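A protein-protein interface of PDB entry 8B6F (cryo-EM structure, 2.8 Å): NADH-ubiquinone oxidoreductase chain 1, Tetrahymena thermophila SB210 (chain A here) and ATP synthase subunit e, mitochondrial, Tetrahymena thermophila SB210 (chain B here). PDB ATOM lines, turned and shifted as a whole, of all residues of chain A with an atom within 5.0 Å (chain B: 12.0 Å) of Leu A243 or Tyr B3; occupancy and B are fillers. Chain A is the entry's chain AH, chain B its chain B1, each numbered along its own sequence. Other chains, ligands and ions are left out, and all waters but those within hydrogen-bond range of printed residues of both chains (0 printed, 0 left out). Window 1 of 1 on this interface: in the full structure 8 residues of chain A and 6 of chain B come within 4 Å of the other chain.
The side-chain hydroxyl (OG) of Ser A95 is in hydrogen-bond range of the backbone carbonyl oxygen (O) of Tyr B3 (3.2 Å).
Ser A95 touches Val B2. Phe A239 touches Tyr B3 (CB to OH, 3.3 Å). CE1 of Tyr A240 touches CE2 of Tyr B3, 3.5 Å away. Tyr A240 touches Gln B4 (OH to CG, 3.7 Å). OH of Tyr A240 touches NZ of Lys B7, 3.9 Å away. Leu A243 touches Tyr B3.
Hydrophobic or aromatic side chains of chain B within 4 Å of the printed part of chain A: Val B2 and Tyr B3. Among the printed residues, no Asp or Glu carboxylate lies within 4 Å of a Lys or Arg side-chain nitrogen of the other chain.
No residue of chain B comes within 4 Å of Pro A94. Printed residues of chain B within 4 Å of Ser A95: Val B2 and Tyr B3. Cys A101 touches none of the printed residues of chain B. Phe A239 touches just one residue of chain B: Tyr B3. Of the printed residues of chain B, Tyr A240 touches Tyr B3, Gln B4 and Lys B7. No residue of chain B comes within 4 Å of Phe A241. No residue of chain B comes within 4 Å of Ala A242. Printed residues of chain B within 4 Å of Leu A243: Tyr B3 (3.8 Å). No residue of chain B comes within 4 Å of Tyr A244. Tyr A245 touches none of the printed residues of chain B. No residue of chain B comes within 4 Å of Gly A247. Of the printed residues of chain A, Val B2 touches Ser A95 (3.6 Å). Of chain A, only Ser A95, Phe A239, Tyr A240 and Leu A243 come within 4 Å of Tyr B3. Of the printed residues of chain A, Gln B4 touches Tyr A240 (3.7 Å). Of the printed residues of chain A, Lys B7 touches Tyr A240 (3.9 Å). The nearest residue of chain B that does not touch Leu A243 is Gln B4 (7.2 Å).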
ATOM      1  N   PRO A  94     -10.836  18.574   0.607  1.00  0.00           N
ATOM      2  CA  PRO A  94     -10.630  19.990   0.260  1.00  0.00           C
ATOM      3  C   PRO A  94      -9.206  20.458   0.484  1.00  0.00           C
ATOM      4  O   PRO A  94      -8.727  21.328  -0.254  1.00  0.00           O
ATOM      5  CB  PRO A  94     -11.628  20.728   1.167  1.00  0.00           C
ATOM      6  CG  PRO A  94     -11.995  19.760   2.227  1.00  0.00           C
ATOM      7  CD  PRO A  94     -11.907  18.407   1.604  1.00  0.00           C
ATOM      8  N   SER A  95      -8.513  19.916   1.486  1.00  0.00           N
ATOM      9  CA  SER A  95      -7.119  20.288   1.704  1.00  0.00           C
ATOM     10  C   SER A  95      -6.258  19.891   0.511  1.00  0.00           C
ATOM     11  O   SER A  95      -5.440  20.681   0.030  1.00  0.00           O
ATOM     12  CB  SER A  95      -6.599  19.636   2.984  1.00  0.00           C
ATOM     13  OG  SER A  95      -5.238  19.962   3.199  1.00  0.00           O
ATOM     14  N   GLY A  98      -7.067  22.173  -2.440  1.00  0.00           N
ATOM     15  CA  GLY A  98      -6.420  23.468  -2.324  1.00  0.00           C
ATOM     16  C   GLY A  98      -4.934  23.400  -2.614  1.00  0.00           C
ATOM     17  O   GLY A  98      -4.379  24.284  -3.269  1.00  0.00           O
ATOM     18  N   CYS A 101      -4.554  23.095  -6.383  1.00  0.00           N
ATOM     19  CA  CYS A 101      -4.903  24.335  -7.069  1.00  0.00           C
ATOM     20  C   CYS A 101      -3.819  25.388  -6.892  1.00  0.00           C
ATOM     21  O   CYS A 101      -3.502  26.125  -7.831  1.00  0.00           O
ATOM     22  CB  CYS A 101      -6.246  24.860  -6.566  1.00  0.00           C
ATOM     23  SG  CYS A 101      -6.173  25.805  -5.032  1.00  0.00           S
ATOM     24  N   TYR A 102      -3.240  25.476  -5.697  1.00  0.00           N
ATOM     25  CA  TYR A 102      -2.152  26.413  -5.458  1.00  0.00           C
ATOM     26  C   TYR A 102      -0.818  25.914  -5.985  1.00  0.00           C
ATOM     27  O   TYR A 102       0.151  26.678  -5.986  1.00  0.00           O
ATOM     28  CB  TYR A 102      -2.039  26.729  -3.967  1.00  0.00           C
ATOM     29  CG  TYR A 102      -2.926  27.875  -3.553  1.00  0.00           C
ATOM     30  CD1 TYR A 102      -2.543  29.185  -3.795  1.00  0.00           C
ATOM     31  CD2 TYR A 102      -4.148  27.650  -2.936  1.00  0.00           C
ATOM     32  CE1 TYR A 102      -3.345  30.241  -3.429  1.00  0.00           C
ATOM     33  CE2 TYR A 102      -4.961  28.703  -2.564  1.00  0.00           C
ATOM     34  CZ  TYR A 102      -4.553  29.996  -2.815  1.00  0.00           C
ATOM     35  OH  TYR A 102      -5.355  31.050  -2.447  1.00  0.00           O
ATOM     36  N   PHE A 239     -14.639  28.206   4.056  1.00  0.00           N
ATOM     37  CA  PHE A 239     -13.413  28.148   3.272  1.00  0.00           C
ATOM     38  C   PHE A 239     -13.235  26.816   2.557  1.00  0.00           C
ATOM     39  O   PHE A 239     -12.461  26.745   1.598  1.00  0.00           O
ATOM     40  CB  PHE A 239     -12.197  28.438   4.149  1.00  0.00           C
ATOM     41  CG  PHE A 239     -10.993  28.868   3.364  1.00  0.00           C
ATOM     42  CD1 PHE A 239     -10.931  30.136   2.813  1.00  0.00           C
ATOM     43  CD2 PHE A 239      -9.932  28.005   3.167  1.00  0.00           C
ATOM     44  CE1 PHE A 239      -9.831  30.535   2.084  1.00  0.00           C
ATOM     45  CE2 PHE A 239      -8.828  28.397   2.439  1.00  0.00           C
ATOM     46  CZ  PHE A 239      -8.777  29.665   1.897  1.00  0.00           C
ATOM     47  N   TYR A 240     -13.921  25.761   2.999  1.00  0.00           N
ATOM     48  CA  TYR A 240     -13.883  24.505   2.257  1.00  0.00           C
ATOM     49  C   TYR A 240     -14.425  24.699   0.847  1.00  0.00           C
ATOM     50  O   TYR A 240     -13.837  24.217  -0.126  1.00  0.00           O
ATOM     51  CB  TYR A 240     -14.678  23.425   2.989  1.00  0.00           C
ATOM     52  CG  TYR A 240     -14.094  22.994   4.318  1.00  0.00           C
ATOM     53  CD1 TYR A 240     -12.869  23.478   4.762  1.00  0.00           C
ATOM     54  CD2 TYR A 240     -14.766  22.086   5.123  1.00  0.00           C
ATOM     55  CE1 TYR A 240     -12.340  23.077   5.972  1.00  0.00           C
ATOM     56  CE2 TYR A 240     -14.245  21.682   6.333  1.00  0.00           C
ATOM     57  CZ  TYR A 240     -13.033  22.179   6.752  1.00  0.00           C
ATOM     58  OH  TYR A 240     -12.514  21.774   7.957  1.00  0.00           O
ATOM     59  N   PHE A 241     -15.544  25.411   0.722  1.00  0.00           N
ATOM     60  CA  PHE A 241     -16.080  25.744  -0.593  1.00  0.00           C
ATOM     61  C   PHE A 241     -15.272  26.843  -1.268  1.00  0.00           C
ATOM     62  O   PHE A 241     -15.148  26.851  -2.497  1.00  0.00           O
ATOM     63  CB  PHE A 241     -17.547  26.152  -0.464  1.00  0.00           C
ATOM     64  CG  PHE A 241     -18.031  27.040  -1.572  1.00  0.00           C
ATOM     65  CD1 PHE A 241     -18.365  26.515  -2.810  1.00  0.00           C
ATOM     66  CD2 PHE A 241     -18.184  28.400  -1.364  1.00  0.00           C
ATOM     67  CE1 PHE A 241     -18.820  27.332  -3.823  1.00  0.00           C
ATOM     68  CE2 PHE A 241     -18.639  29.223  -2.373  1.00  0.00           C
ATOM     69  CZ  PHE A 241     -18.960  28.688  -3.604  1.00  0.00           C
ATOM     70  N   ALA A 242     -14.712  27.772  -0.493  1.00  0.00           N
ATOM     71  CA  ALA A 242     -13.852  28.795  -1.079  1.00  0.00           C
ATOM     72  C   ALA A 242     -12.672  28.167  -1.804  1.00  0.00           C
ATOM     73  O   ALA A 242     -12.249  28.656  -2.858  1.00  0.00           O
ATOM     74  CB  ALA A 242     -13.347  29.743   0.005  1.00  0.00           C
ATOM     75  N   LEU A 243     -12.128  27.079  -1.257  1.00  0.00           N
ATOM     76  CA  LEU A 243     -11.003  26.412  -1.902  1.00  0.00           C
ATOM     77  C   LEU A 243     -11.395  25.861  -3.265  1.00  0.00           C
ATOM     78  O   LEU A 243     -10.638  25.989  -4.233  1.00  0.00           O
ATOM     79  CB  LEU A 243     -10.469  25.297  -1.004  1.00  0.00           C
ATOM     80  CG  LEU A 243      -9.660  25.740   0.218  1.00  0.00           C
ATOM     81  CD1 LEU A 243      -9.353  24.559   1.117  1.00  0.00           C
ATOM     82  CD2 LEU A 243      -8.371  26.426  -0.209  1.00  0.00           C
ATOM     83  N   TYR A 244     -12.568  25.238  -3.364  1.00  0.00           N
ATOM     84  CA  TYR A 244     -13.013  24.732  -4.657  1.00  0.00           C
ATOM     85  C   TYR A 244     -13.220  25.869  -5.649  1.00  0.00           C
ATOM     86  O   TYR A 244     -12.840  25.757  -6.821  1.00  0.00           O
ATOM     87  CB  TYR A 244     -14.300  23.929  -4.488  1.00  0.00           C
ATOM     88  CG  TYR A 244     -14.115  22.649  -3.713  1.00  0.00           C
ATOM     89  CD1 TYR A 244     -13.482  21.554  -4.285  1.00  0.00           C
ATOM     90  CD2 TYR A 244     -14.581  22.530  -2.412  1.00  0.00           C
ATOM     91  CE1 TYR A 244     -13.314  20.381  -3.583  1.00  0.00           C
ATOM     92  CE2 TYR A 244     -14.418  21.362  -1.701  1.00  0.00           C
ATOM     93  CZ  TYR A 244     -13.784  20.291  -2.291  1.00  0.00           C
ATOM     94  OH  TYR A 244     -13.619  19.123  -1.586  1.00  0.00           O
ATOM     95  N   TYR A 245     -13.820  26.974  -5.201  1.00  0.00           N
ATOM     96  CA  TYR A 245     -14.013  28.117  -6.087  1.00  0.00           C
ATOM     97  C   TYR A 245     -12.676  28.672  -6.559  1.00  0.00           C
ATOM     98  O   TYR A 245     -12.508  28.989  -7.742  1.00  0.00           O
ATOM     99  CB  TYR A 245     -14.819  29.203  -5.375  1.00  0.00           C
ATOM    100  CG  TYR A 245     -16.048  29.650  -6.128  1.00  0.00           C
ATOM    101  CD1 TYR A 245     -17.127  28.795  -6.302  1.00  0.00           C
ATOM    102  CD2 TYR A 245     -16.138  30.934  -6.648  1.00  0.00           C
ATOM    103  CE1 TYR A 245     -18.258  29.201  -6.984  1.00  0.00           C
ATOM    104  CE2 TYR A 245     -17.264  31.351  -7.332  1.00  0.00           C
ATOM    105  CZ  TYR A 245     -18.321  30.480  -7.496  1.00  0.00           C
ATOM    106  OH  TYR A 245     -19.445  30.889  -8.174  1.00  0.00           O
ATOM    107  N   LEU A 246     -11.713  28.799  -5.645  1.00  0.00           N
ATOM    108  CA  LEU A 246     -10.391  29.289  -6.020  1.00  0.00           C
ATOM    109  C   LEU A 246      -9.728  28.361  -7.026  1.00  0.00           C
ATOM    110  O   LEU A 246      -9.093  28.820  -7.983  1.00  0.00           O
ATOM    111  CB  LEU A 246      -9.513  29.440  -4.778  1.00  0.00           C
ATOM    112  CG  LEU A 246      -9.860  30.581  -3.818  1.00  0.00           C
ATOM    113  CD1 LEU A 246      -8.990  30.507  -2.580  1.00  0.00           C
ATOM    114  CD2 LEU A 246      -9.702  31.935  -4.493  1.00  0.00           C
ATOM    115  N   GLY A 247      -9.868  27.051  -6.832  1.00  0.00           N
ATOM    116  CA  GLY A 247      -9.285  26.115  -7.777  1.00  0.00           C
ATOM    117  C   GLY A 247      -9.913  26.208  -9.151  1.00  0.00           C
ATOM    118  O   GLY A 247      -9.218  26.147 -10.167  1.00  0.00           O
ATOM    119  N   VAL B   2      -0.252  22.330   5.536  1.00  0.00           N
ATOM    120  CA  VAL B   2      -1.490  21.543   5.302  1.00  0.00           C
ATOM    121  C   VAL B   2      -2.665  22.285   5.910  1.00  0.00           C
ATOM    122  O   VAL B   2      -2.732  22.461   7.124  1.00  0.00           O
ATOM    123  CB  VAL B   2      -1.379  20.117   5.884  1.00  0.00           C
ATOM    124  CG1 VAL B   2      -2.642  19.322   5.596  1.00  0.00           C
ATOM    125  CG2 VAL B   2      -0.169  19.393   5.320  1.00  0.00           C
ATOM    126  N   TYR B   3      -3.592  22.729   5.065  1.00  0.00           N
ATOM    127  CA  TYR B   3      -4.802  23.358   5.571  1.00  0.00           C
ATOM    128  C   TYR B   3      -5.562  22.368   6.441  1.00  0.00           C
ATOM    129  O   TYR B   3      -5.775  21.217   6.051  1.00  0.00           O
ATOM    130  CB  TYR B   3      -5.676  23.836   4.411  1.00  0.00           C
ATOM    131  CG  TYR B   3      -6.938  24.534   4.856  1.00  0.00           C
ATOM    132  CD1 TYR B   3      -6.890  25.792   5.438  1.00  0.00           C
ATOM    133  CD2 TYR B   3      -8.179  23.937   4.686  1.00  0.00           C
ATOM    134  CE1 TYR B   3      -8.041  26.433   5.846  1.00  0.00           C
ATOM    135  CE2 TYR B   3      -9.334  24.569   5.090  1.00  0.00           C
ATOM    136  CZ  TYR B   3      -9.260  25.816   5.670  1.00  0.00           C
ATOM    137  OH  TYR B   3     -10.410  26.449   6.072  1.00  0.00           O
ATOM    138  N   GLN B   4      -5.969  22.818   7.626  1.00  0.00           N
ATOM    139  CA  GLN B   4      -6.568  21.938   8.624  1.00  0.00           C
ATOM    140  C   GLN B   4      -5.653  20.747   8.894  1.00  0.00           C
ATOM    141  O   GLN B   4      -6.081  19.593   8.941  1.00  0.00           O
ATOM    142  CB  GLN B   4      -7.957  21.475   8.184  1.00  0.00           C
ATOM    143  CG  GLN B   4      -8.942  22.612   7.989  1.00  0.00           C
ATOM    144  CD  GLN B   4      -9.220  23.368   9.268  1.00  0.00           C
ATOM    145  OE1 GLN B   4      -8.939  22.885  10.362  1.00  0.00           O
ATOM    146  NE2 GLN B   4      -9.774  24.567   9.137  1.00  0.00           N
ATOM    147  N   GLY B   5      -4.367  21.047   9.085  1.00  0.00           N
ATOM    148  CA  GLY B   5      -3.388  19.989   9.269  1.00  0.00           C
ATOM    149  C   GLY B   5      -3.692  19.099  10.458  1.00  0.00           C
ATOM    150  O   GLY B   5      -3.498  17.883  10.399  1.00  0.00           O
ATOM    151  N   PHE B   6      -4.168  19.687  11.554  1.00  0.00           N
ATOM    152  CA  PHE B   6      -4.478  18.888  12.735  1.00  0.00           C
ATOM    153  C   PHE B   6      -5.643  17.945  12.465  1.00  0.00           C
ATOM    154  O   PHE B   6      -5.548  16.740  12.718  1.00  0.00           O
ATOM    155  CB  PHE B   6      -4.786  19.798  13.922  1.00  0.00           C
ATOM    156  CG  PHE B   6      -5.134  19.048  15.174  1.00  0.00           C
ATOM    157  CD1 PHE B   6      -4.152  18.400  15.903  1.00  0.00           C
ATOM    158  CD2 PHE B   6      -6.440  18.988  15.620  1.00  0.00           C
ATOM    159  CE1 PHE B   6      -4.469  17.708  17.053  1.00  0.00           C
ATOM    160  CE2 PHE B   6      -6.762  18.296  16.768  1.00  0.00           C
ATOM    161  CZ  PHE B   6      -5.776  17.656  17.486  1.00  0.00           C
ATOM    162  N   LYS B   7      -6.747  18.470  11.928  1.00  0.00           N
ATOM    163  CA  LYS B   7      -7.883  17.614  11.609  1.00  0.00           C
ATOM    164  C   LYS B   7      -7.504  16.530  10.610  1.00  0.00           C
ATOM    165  O   LYS B   7      -8.110  15.452  10.605  1.00  0.00           O
ATOM    166  CB  LYS B   7      -9.035  18.450  11.054  1.00  0.00           C
ATOM    167  CG  LYS B   7      -9.601  19.458  12.036  1.00  0.00           C
ATOM    168  CD  LYS B   7     -10.802  20.176  11.446  1.00  0.00           C
ATOM    169  CE  LYS B   7     -11.330  21.230  12.398  1.00  0.00           C
ATOM    170  NZ  LYS B   7     -12.504  21.950  11.836  1.00  0.00           N
ATOM    171  N   VAL B   8      -6.518  16.795   9.756  1.00  0.00           N
ATOM    172  CA  VAL B   8      -6.123  15.820   8.745  1.00  0.00           C
ATOM    173  C   VAL B   8      -5.217  14.751   9.345  1.00  0.00           C
ATOM    174  O   VAL B   8      -5.288  13.579   8.961  1.00  0.00           O
ATOM    175  CB  VAL B   8      -5.451  16.540   7.563  1.00  0.00           C
ATOM    176  CG1 VAL B   8      -4.814  15.546   6.610  1.00  0.00           C
ATOM    177  CG2 VAL B   8      -6.464  17.388   6.818  1.00  0.00           C
ATOM    178  N   LEU B   9      -4.355  15.129  10.287  1.00  0.00           N
ATOM    179  CA  LEU B   9      -3.356  14.226  10.841  1.00  0.00           C
ATOM    180  C   LEU B   9      -3.744  13.661  12.203  1.00  0.00           C
ATOM    181  O   LEU B   9      -2.921  12.998  12.839  1.00  0.00           O
ATOM    182  CB  LEU B   9      -2.008  14.943  10.941  1.00  0.00           C
ATOM    183  CG  LEU B   9      -1.367  15.363   9.617  1.00  0.00           C
ATOM    184  CD1 LEU B   9      -0.136  16.213   9.857  1.00  0.00           C
ATOM    185  CD2 LEU B   9      -1.006  14.146   8.784  1.00  0.00           C
ATOM    186  N   ARG B  10      -4.968  13.910  12.670  1.00  0.00           N
ATOM    187  CA  ARG B  10      -5.389  13.362  13.956  1.00  0.00           C
ATOM    188  C   ARG B  10      -5.314  11.841  13.960  1.00  0.00           C
ATOM    189  O   ARG B  10      -4.700  11.239  14.849  1.00  0.00           O
ATOM    190  CB  ARG B  10      -6.814  13.816  14.278  1.00  0.00           C
ATOM    191  CG  ARG B  10      -6.903  15.105  15.074  1.00  0.00           C
ATOM    192  CD  ARG B  10      -8.345  15.455  15.426  1.00  0.00           C
ATOM    193  NE  ARG B  10      -9.234  15.422  14.271  1.00  0.00           N
ATOM    194  CZ  ARG B  10     -10.406  16.039  14.207  1.00  0.00           C
ATOM    195  NH1 ARG B  10     -10.850  16.785  15.203  1.00  0.00           N
ATOM    196  NH2 ARG B  10     -11.149  15.907  13.113  1.00  0.00           N
